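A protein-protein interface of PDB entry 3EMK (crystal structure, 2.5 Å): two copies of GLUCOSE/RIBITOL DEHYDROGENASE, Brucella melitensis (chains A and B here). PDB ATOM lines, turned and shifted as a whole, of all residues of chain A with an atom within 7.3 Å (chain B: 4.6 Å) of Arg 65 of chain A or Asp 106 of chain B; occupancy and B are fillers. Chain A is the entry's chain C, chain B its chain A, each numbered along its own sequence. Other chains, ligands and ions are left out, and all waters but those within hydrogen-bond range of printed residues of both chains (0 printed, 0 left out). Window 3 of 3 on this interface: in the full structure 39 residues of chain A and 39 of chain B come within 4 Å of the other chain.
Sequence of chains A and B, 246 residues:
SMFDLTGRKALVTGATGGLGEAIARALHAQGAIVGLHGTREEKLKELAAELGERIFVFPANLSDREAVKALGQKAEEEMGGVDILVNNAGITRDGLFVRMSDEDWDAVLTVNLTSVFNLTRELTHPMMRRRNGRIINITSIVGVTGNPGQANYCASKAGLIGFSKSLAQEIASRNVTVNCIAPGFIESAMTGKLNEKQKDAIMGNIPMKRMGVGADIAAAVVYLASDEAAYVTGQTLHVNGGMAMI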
ATOM      1  N   ASN A  61     -24.954  11.434 -12.350  1.00  0.00           N
ATOM      2  CA  ASN A  61     -26.184  11.675 -11.612  1.00  0.00           C
ATOM      3  C   ASN A  61     -26.120  10.907 -10.298  1.00  0.00           C
ATOM      4  O   ASN A  61     -26.257   9.685 -10.275  1.00  0.00           O
ATOM      5  CB  ASN A  61     -27.383  11.244 -12.458  1.00  0.00           C
ATOM      6  CG  ASN A  61     -28.705  11.482 -11.778  1.00  0.00           C
ATOM      7  OD1 ASN A  61     -29.737  11.082 -12.316  1.00  0.00           O
ATOM      8  ND2 ASN A  61     -28.706  12.140 -10.610  1.00  0.00           N
ATOM      9  N   LEU A  62     -25.903  11.633  -9.209  1.00  0.00           N
ATOM     10  CA  LEU A  62     -25.704  11.023  -7.897  1.00  0.00           C
ATOM     11  C   LEU A  62     -26.970  10.396  -7.285  1.00  0.00           C
ATOM     12  O   LEU A  62     -26.903   9.743  -6.238  1.00  0.00           O
ATOM     13  CB  LEU A  62     -25.049  12.024  -6.935  1.00  0.00           C
ATOM     14  CG  LEU A  62     -23.668  12.561  -7.338  1.00  0.00           C
ATOM     15  CD1 LEU A  62     -23.206  13.647  -6.392  1.00  0.00           C
ATOM     16  CD2 LEU A  62     -22.637  11.451  -7.398  1.00  0.00           C
ATOM     17  N   SER A  63     -28.118  10.596  -7.934  1.00  0.00           N
ATOM     18  CA  SER A  63     -29.361   9.933  -7.509  1.00  0.00           C
ATOM     19  C   SER A  63     -29.390   8.500  -8.035  1.00  0.00           C
ATOM     20  O   SER A  63     -30.265   7.712  -7.669  1.00  0.00           O
ATOM     21  CB  SER A  63     -30.599  10.696  -7.988  1.00  0.00           C
ATOM     22  OG  SER A  63     -30.854  11.807  -7.159  1.00  0.00           O
ATOM     23  N   ASP A  64     -28.413   8.185  -8.880  1.00  0.00           N
ATOM     24  CA  ASP A  64     -28.341   6.910  -9.578  1.00  0.00           C
ATOM     25  C   ASP A  64     -27.210   6.077  -9.000  1.00  0.00           C
ATOM     26  O   ASP A  64     -26.040   6.351  -9.259  1.00  0.00           O
ATOM     27  CB  ASP A  64     -28.156   7.146 -11.095  1.00  0.00           C
ATOM     28  CG  ASP A  64     -28.070   5.848 -11.887  1.00  0.00           C
ATOM     29  OD1 ASP A  64     -27.189   5.004 -11.614  1.00  0.00           O
ATOM     30  OD2 ASP A  64     -28.891   5.660 -12.797  1.00  0.00           O
ATOM     31  N   ARG A  65     -27.568   5.062  -8.220  1.00  0.00           N
ATOM     32  CA  ARG A  65     -26.598   4.244  -7.508  1.00  0.00           C
ATOM     33  C   ARG A  65     -25.487   3.785  -8.459  1.00  0.00           C
ATOM     34  O   ARG A  65     -24.316   4.025  -8.200  1.00  0.00           O
ATOM     35  CB  ARG A  65     -27.303   3.072  -6.794  1.00  0.00           C
ATOM     36  CG  ARG A  65     -26.407   1.894  -6.386  1.00  0.00           C
ATOM     37  CD  ARG A  65     -25.946   1.971  -4.950  1.00  0.00           C
ATOM     38  NE  ARG A  65     -27.012   1.581  -4.033  1.00  0.00           N
ATOM     39  CZ  ARG A  65     -26.943   1.660  -2.710  1.00  0.00           C
ATOM     40  NH1 ARG A  65     -25.858   2.103  -2.123  1.00  0.00           N
ATOM     41  NH2 ARG A  65     -27.966   1.291  -1.970  1.00  0.00           N
ATOM     42  N   GLU A  66     -25.871   3.176  -9.576  1.00  0.00           N
ATOM     43  CA  GLU A  66     -24.923   2.638 -10.556  1.00  0.00           C
ATOM     44  C   GLU A  66     -23.974   3.672 -11.184  1.00  0.00           C
ATOM     45  O   GLU A  66     -22.809   3.361 -11.448  1.00  0.00           O
ATOM     46  CB  GLU A  66     -25.674   1.858 -11.644  1.00  0.00           C
ATOM     47  CG  GLU A  66     -24.757   1.257 -12.712  1.00  0.00           C
ATOM     48  CD  GLU A  66     -24.829  -0.272 -12.750  1.00  0.00           C
ATOM     49  OE1 GLU A  66     -24.769  -0.835 -13.876  1.00  0.00           O
ATOM     50  OE2 GLU A  66     -24.941  -0.901 -11.655  1.00  0.00           O
ATOM     51  N   ALA A  67     -24.476   4.889 -11.419  1.00  0.00           N
ATOM     52  CA  ALA A  67     -23.641   5.989 -11.894  1.00  0.00           C
ATOM     53  C   ALA A  67     -22.640   6.438 -10.819  1.00  0.00           C
ATOM     54  O   ALA A  67     -21.507   6.800 -11.144  1.00  0.00           O
ATOM     55  CB  ALA A  67     -24.491   7.158 -12.373  1.00  0.00           C
ATOM     56  N   VAL A  68     -23.051   6.401  -9.547  1.00  0.00           N
ATOM     57  CA  VAL A  68     -22.146   6.711  -8.431  1.00  0.00           C
ATOM     58  C   VAL A  68     -20.937   5.769  -8.447  1.00  0.00           C
ATOM     59  O   VAL A  68     -19.789   6.221  -8.470  1.00  0.00           O
ATOM     60  CB  VAL A  68     -22.843   6.640  -7.043  1.00  0.00           C
ATOM     61  CG1 VAL A  68     -21.838   6.910  -5.944  1.00  0.00           C
ATOM     62  CG2 VAL A  68     -24.009   7.627  -6.959  1.00  0.00           C
ATOM     63  N   LYS A  69     -21.210   4.461  -8.450  1.00  0.00           N
ATOM     64  CA  LYS A  69     -20.149   3.456  -8.505  1.00  0.00           C
ATOM     65  C   LYS A  69     -19.262   3.643  -9.718  1.00  0.00           C
ATOM     66  O   LYS A  69     -18.050   3.510  -9.618  1.00  0.00           O
ATOM     67  CB  LYS A  69     -20.714   2.042  -8.519  1.00  0.00           C
ATOM     68  CG  LYS A  69     -21.321   1.589  -7.220  1.00  0.00           C
ATOM     69  CD  LYS A  69     -22.138   0.318  -7.429  1.00  0.00           C
ATOM     70  CE  LYS A  69     -23.177   0.204  -6.346  1.00  0.00           C
ATOM     71  NZ  LYS A  69     -23.215  -1.135  -5.802  1.00  0.00           N
ATOM     72  N   ALA A  70     -19.868   3.961 -10.861  1.00  0.00           N
ATOM     73  CA  ALA A  70     -19.117   4.131 -12.106  1.00  0.00           C
ATOM     74  C   ALA A  70     -18.227   5.384 -12.040  1.00  0.00           C
ATOM     75  O   ALA A  70     -17.122   5.388 -12.584  1.00  0.00           O
ATOM     76  CB  ALA A  70     -20.061   4.182 -13.293  1.00  0.00           C
ATOM     77  N   LEU A  71     -18.701   6.429 -11.358  1.00  0.00           N
ATOM     78  CA  LEU A  71     -17.880   7.615 -11.086  1.00  0.00           C
ATOM     79  C   LEU A  71     -16.592   7.208 -10.358  1.00  0.00           C
ATOM     80  O   LEU A  71     -15.495   7.560 -10.788  1.00  0.00           O
ATOM     81  CB  LEU A  71     -18.658   8.669 -10.269  1.00  0.00           C
ATOM     82  CG  LEU A  71     -18.350  10.186 -10.325  1.00  0.00           C
ATOM     83  CD1 LEU A  71     -18.702  10.891  -8.995  1.00  0.00           C
ATOM     84  CD2 LEU A  71     -16.921  10.510 -10.719  1.00  0.00           C
ATOM     85  N   THR A 114     -26.454   8.326   1.219  1.00  0.00           N
ATOM     86  CA  THR A 114     -26.135   7.032   0.601  1.00  0.00           C
ATOM     87  C   THR A 114     -25.284   7.068  -0.700  1.00  0.00           C
ATOM     88  O   THR A 114     -24.650   6.075  -1.045  1.00  0.00           O
ATOM     89  CB  THR A 114     -27.324   5.982   0.615  1.00  0.00           C
ATOM     90  OG1 THR A 114     -27.488   5.375  -0.680  1.00  0.00           O
ATOM     91  CG2 THR A 114     -28.615   6.571   1.124  1.00  0.00           C
ATOM     92  N   SER A 115     -25.232   8.205  -1.391  1.00  0.00           N
ATOM     93  CA  SER A 115     -24.364   8.280  -2.563  1.00  0.00           C
ATOM     94  C   SER A 115     -22.941   8.600  -2.107  1.00  0.00           C
ATOM     95  O   SER A 115     -21.960   8.254  -2.799  1.00  0.00           O
ATOM     96  CB  SER A 115     -24.877   9.266  -3.625  1.00  0.00           C
ATOM     97  OG  SER A 115     -24.571  10.614  -3.300  1.00  0.00           O
ATOM     98  N   PHE A 117     -21.889   7.249   0.824  1.00  0.00           N
ATOM     99  CA  PHE A 117     -21.560   5.866   1.166  1.00  0.00           C
ATOM    100  C   PHE A 117     -20.898   5.231  -0.050  1.00  0.00           C
ATOM    101  O   PHE A 117     -19.688   4.965  -0.011  1.00  0.00           O
ATOM    102  CB  PHE A 117     -22.800   5.089   1.661  1.00  0.00           C
ATOM    103  CG  PHE A 117     -22.615   3.576   1.725  1.00  0.00           C
ATOM    104  CD1 PHE A 117     -21.832   2.986   2.721  1.00  0.00           C
ATOM    105  CD2 PHE A 117     -23.250   2.735   0.793  1.00  0.00           C
ATOM    106  CE1 PHE A 117     -21.667   1.592   2.792  1.00  0.00           C
ATOM    107  CE2 PHE A 117     -23.086   1.335   0.843  1.00  0.00           C
ATOM    108  CZ  PHE A 117     -22.289   0.767   1.850  1.00  0.00           C
ATOM    109  N   ASN A 118     -21.649   5.062  -1.143  1.00  0.00           N
ATOM    110  CA  ASN A 118     -21.110   4.406  -2.341  1.00  0.00           C
ATOM    111  C   ASN A 118     -19.781   4.982  -2.848  1.00  0.00           C
ATOM    112  O   ASN A 118     -18.792   4.251  -2.960  1.00  0.00           O
ATOM    113  CB  ASN A 118     -22.134   4.373  -3.477  1.00  0.00           C
ATOM    114  CG  ASN A 118     -23.312   3.494  -3.167  1.00  0.00           C
ATOM    115  OD1 ASN A 118     -23.164   2.289  -2.986  1.00  0.00           O
ATOM    116  ND2 ASN A 118     -24.496   4.087  -3.126  1.00  0.00           N
ATOM    117  N   LEU A 119     -19.744   6.279  -3.146  1.00  0.00           N
ATOM    118  CA  LEU A 119     -18.524   6.856  -3.666  1.00  0.00           C
ATOM    119  C   LEU A 119     -17.345   6.509  -2.767  1.00  0.00           C
ATOM    120  O   LEU A 119     -16.324   6.009  -3.244  1.00  0.00           O
ATOM    121  CB  LEU A 119     -18.633   8.369  -3.796  1.00  0.00           C
ATOM    122  CG  LEU A 119     -18.223   8.896  -5.177  1.00  0.00           C
ATOM    123  CD1 LEU A 119     -17.932  10.379  -5.109  1.00  0.00           C
ATOM    124  CD2 LEU A 119     -17.069   8.134  -5.793  1.00  0.00           C
ATOM    125  N   ARG A 121     -17.049   4.165  -0.583  1.00  0.00           N
ATOM    126  CA  ARG A 121     -16.788   2.732  -0.652  1.00  0.00           C
ATOM    127  C   ARG A 121     -16.030   2.300  -1.917  1.00  0.00           C
ATOM    128  O   ARG A 121     -15.392   1.252  -1.942  1.00  0.00           O
ATOM    129  CB  ARG A 121     -18.074   1.928  -0.513  1.00  0.00           C
ATOM    130  CG  ARG A 121     -17.822   0.519   0.029  1.00  0.00           C
ATOM    131  CD  ARG A 121     -19.051  -0.358  -0.104  1.00  0.00           C
ATOM    132  NE  ARG A 121     -19.319  -0.676  -1.504  1.00  0.00           N
ATOM    133  CZ  ARG A 121     -20.447  -1.214  -1.950  1.00  0.00           C
ATOM    134  NH1 ARG A 121     -21.455  -1.513  -1.115  1.00  0.00           N
ATOM    135  NH2 ARG A 121     -20.569  -1.447  -3.238  1.00  0.00           N
ATOM    136  N   GLU A 122     -16.101   3.110  -2.960  1.00  0.00           N
ATOM    137  CA  GLU A 122     -15.416   2.787  -4.197  1.00  0.00           C
ATOM    138  C   GLU A 122     -13.893   3.062  -4.051  1.00  0.00           C
ATOM    139  O   GLU A 122     -13.066   2.352  -4.638  1.00  0.00           O
ATOM    140  CB  GLU A 122     -16.061   3.606  -5.322  1.00  0.00           C
ATOM    141  CG  GLU A 122     -16.388   2.891  -6.598  1.00  0.00           C
ATOM    142  CD  GLU A 122     -17.019   1.535  -6.410  1.00  0.00           C
ATOM    143  OE1 GLU A 122     -18.199   1.446  -6.019  1.00  0.00           O
ATOM    144  OE2 GLU A 122     -16.331   0.544  -6.705  1.00  0.00           O
ATOM    145  N   ASP B 102     -24.452  -2.851  -0.199  1.00  0.00           N
ATOM    146  CA  ASP B 102     -25.560  -1.905  -0.327  1.00  0.00           C
ATOM    147  C   ASP B 102     -26.729  -2.313   0.548  1.00  0.00           C
ATOM    148  O   ASP B 102     -27.357  -1.473   1.190  1.00  0.00           O
ATOM    149  CB  ASP B 102     -26.040  -1.795  -1.778  1.00  0.00           C
ATOM    150  CG  ASP B 102     -24.953  -1.334  -2.732  1.00  0.00           C
ATOM    151  OD1 ASP B 102     -23.986  -0.635  -2.332  1.00  0.00           O
ATOM    152  OD2 ASP B 102     -25.074  -1.666  -3.922  1.00  0.00           O
ATOM    153  N   GLU B 103     -27.013  -3.611   0.558  1.00  0.00           N
ATOM    154  CA  GLU B 103     -28.172  -4.156   1.256  1.00  0.00           C
ATOM    155  C   GLU B 103     -28.032  -3.920   2.767  1.00  0.00           C
ATOM    156  O   GLU B 103     -29.014  -3.639   3.447  1.00  0.00           O
ATOM    157  CB  GLU B 103     -28.323  -5.643   0.931  1.00  0.00           C
ATOM    158  CG  GLU B 103     -29.492  -6.335   1.624  1.00  0.00           C
ATOM    159  CD  GLU B 103     -29.347  -7.877   1.713  1.00  0.00           C
ATOM    160  OE1 GLU B 103     -28.375  -8.462   1.152  1.00  0.00           O
ATOM    161  OE2 GLU B 103     -30.223  -8.507   2.360  1.00  0.00           O
ATOM    162  N   ASP B 104     -26.802  -4.012   3.267  1.00  0.00           N
ATOM    163  CA  ASP B 104     -26.502  -3.770   4.681  1.00  0.00           C
ATOM    164  C   ASP B 104     -26.588  -2.295   5.094  1.00  0.00           C
ATOM    165  O   ASP B 104     -26.896  -1.982   6.241  1.00  0.00           O
ATOM    166  CB  ASP B 104     -25.125  -4.340   5.047  1.00  0.00           C
ATOM    167  CG  ASP B 104     -25.144  -5.841   5.226  1.00  0.00           C
ATOM    168  OD1 ASP B 104     -26.240  -6.440   5.340  1.00  0.00           O
ATOM    169  OD2 ASP B 104     -24.044  -6.419   5.266  1.00  0.00           O
ATOM    170  N   TRP B 105     -26.304  -1.400   4.158  1.00  0.00           N
ATOM    171  CA  TRP B 105     -26.411   0.026   4.398  1.00  0.00           C
ATOM    172  C   TRP B 105     -27.894   0.374   4.312  1.00  0.00           C
ATOM    173  O   TRP B 105     -28.485   0.865   5.300  1.00  0.00           O
ATOM    174  CB  TRP B 105     -25.552   0.804   3.386  1.00  0.00           C
ATOM    175  CG  TRP B 105     -25.790   2.261   3.395  1.00  0.00           C
ATOM    176  CD1 TRP B 105     -26.708   2.936   2.646  1.00  0.00           C
ATOM    177  CD2 TRP B 105     -25.129   3.247   4.205  1.00  0.00           C
ATOM    178  NE1 TRP B 105     -26.660   4.275   2.933  1.00  0.00           N
ATOM    179  CE2 TRP B 105     -25.705   4.497   3.890  1.00  0.00           C
ATOM    180  CE3 TRP B 105     -24.103   3.197   5.165  1.00  0.00           C
ATOM    181  CZ2 TRP B 105     -25.288   5.698   4.500  1.00  0.00           C
ATOM    182  CZ3 TRP B 105     -23.689   4.390   5.773  1.00  0.00           C
ATOM    183  CH2 TRP B 105     -24.285   5.619   5.439  1.00  0.00           C
ATOM    184  N   ASP B 106     -28.513   0.056   3.169  1.00  0.00           N
ATOM    185  CA  ASP B 106     -29.946   0.321   2.975  1.00  0.00           C
ATOM    186  C   ASP B 106     -30.831  -0.105   4.135  1.00  0.00           C
ATOM    187  O   ASP B 106     -31.485   0.749   4.726  1.00  0.00           O
ATOM    188  CB  ASP B 106     -30.472  -0.243   1.660  1.00  0.00           C
ATOM    189  CG  ASP B 106     -29.830   0.412   0.453  1.00  0.00           C
ATOM    190  OD1 ASP B 106     -29.173   1.458   0.597  1.00  0.00           O
ATOM    191  OD2 ASP B 106     -29.976  -0.132  -0.657  1.00  0.00           O
ATOM    192  N   ALA B 107     -30.835  -1.398   4.474  1.00  0.00           N
ATOM    193  CA  ALA B 107     -31.707  -1.933   5.534  1.00  0.00           C
ATOM    194  C   ALA B 107     -31.625  -1.132   6.837  1.00  0.00           C
ATOM    195  O   ALA B 107     -32.644  -0.835   7.437  1.00  0.00           O
ATOM    196  CB  ALA B 107     -31.391  -3.424   5.808  1.00  0.00           C
ATOM    197  N   VAL B 108     -30.401  -0.795   7.257  1.00  0.00           N
ATOM    198  CA  VAL B 108     -30.139   0.003   8.461  1.00  0.00           C
ATOM    199  C   VAL B 108     -30.710   1.426   8.373  1.00  0.00           C
ATOM    200  O   VAL B 108     -31.301   1.914   9.335  1.00  0.00           O
ATOM    201  CB  VAL B 108     -28.625   0.027   8.789  1.00  0.00           C
ATOM    202  CG1 VAL B 108     -28.273   1.116   9.822  1.00  0.00           C
ATOM    203  CG2 VAL B 108     -28.169  -1.367   9.247  1.00  0.00           C
ATOM    204  N   LEU B 109     -30.544   2.074   7.222  1.00  0.00           N
ATOM    205  CA  LEU B 109     -31.079   3.419   7.008  1.00  0.00           C
ATOM    206  C   LEU B 109     -32.585   3.374   6.999  1.00  0.00           C
ATOM    207  O   LEU B 109     -33.254   4.095   7.763  1.00  0.00           O
ATOM    208  CB  LEU B 109     -30.580   4.016   5.692  1.00  0.00           C
ATOM    209  CG  LEU B 109     -29.338   4.889   5.815  1.00  0.00           C
ATOM    210  CD1 LEU B 109     -29.698   6.192   6.527  1.00  0.00           C
ATOM    211  CD2 LEU B 109     -28.219   4.159   6.588  1.00  0.00           C
ATOM    212  N   THR B 110     -33.121   2.492   6.161  1.00  0.00           N
ATOM    213  CA  THR B 110     -34.557   2.419   6.029  1.00  0.00           C
ATOM    214  C   THR B 110     -35.229   2.054   7.360  1.00  0.00           C
ATOM    215  O   THR B 110     -36.256   2.647   7.663  1.00  0.00           O
ATOM    216  CB  THR B 110     -35.080   1.576   4.800  1.00  0.00           C
ATOM    217  OG1 THR B 110     -35.419   0.259   5.220  1.00  0.00           O
ATOM    218  CG2 THR B 110     -34.098   1.545   3.628  1.00  0.00           C
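The guanidinium group of Arg 65 of chain A sits close to the side-chain amide nitrogen of Asn 118 of chain A, at 2.6 Å. The side-chain amide nitrogen (ND2) of Asn 118 of chain A sits at hydrogen-bond distance from the backbone carbonyl oxygen (O) of Thr 114 of chain A, 2.9 Å away.
Trp 105 of chain B touches Thr 114 of chain A (NE1 to CB, 3.0 Å). Phe 117 of chain A touches Asp 102 of chain B. Phe 117 of chain A touches Trp 105 of chain B.
No position is printed for both chains. Of the 8 pairs that touch across the chains among the printed residues, none has its exchanged pair printed and touching as well.
Printed residues of chain A that touch a printed residue of chain B: Arg 65, Lys 69, Thr 114, Phe 117, Asn 118 and Arg 121. Hydrophobic or aromatic side chains of chain A within 4 Å of the printed part of chain B: Phe 117. Hydrophobic or aromatic side chains of chain B within 4 Å of the printed part of chain A: Trp 105. Among the printed residues, Asp or Glu carboxylates within 4 Å of a Lys or Arg side-chain nitrogen of the other chain: Arg 65 of chain A with Asp 102 of chain B, Arg 65 of chain A with Asp 106 of chain B, Lys 69 of chain A with Asp 102 of chain B and Arg 121 of chain A with Asp 102 of chain B.
Printed residues of chain B within 4 Å of Arg 65 of chain A: Asp 102 and Asp 106. Printed residues of chain B within 4 Å of Thr 114 of chain A: Trp 105 (3.0 Å). Of the printed residues of chain B, Asn 118 of chain A touches Asp 102. Asp 106 of chain B touches one residue of chain A. The nearest residue of chain A that does not touch Asp 106 of chain B is Thr 114 of chain A (4.5 Å). The nearest printed residue of chain A that does not touch Trp 105 of chain B is Arg 65 of chain A (4.9 Å).
The guanidinium group of Arg 65 of chain A is in salt-bridge range of the side-chain carboxylate of Asp 102 of chain B. The side-chain carboxylate (OD2) of Asp 102 of chain B lies within salt-bridge range of the side-chain amino group (NZ) of Lys 69 of chain A, 2.7 Å away. The side-chain carboxylate (OD1) of Asp 102 of chain B sits close to the side-chain amide oxygen (OD1) of Asn 118 of chain A, 3.1 Å away. The side-chain carboxylate of Asp 102 of chain B lies within salt-bridge range of the guanidinium group of Arg 121 of chain A (2.9 Å). The side-chain carboxylate (OD2) of Asp 106 of chain B lies within salt-bridge range of the guanidinium group (NH2) of Arg 65 of chain A (2.8 Å).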
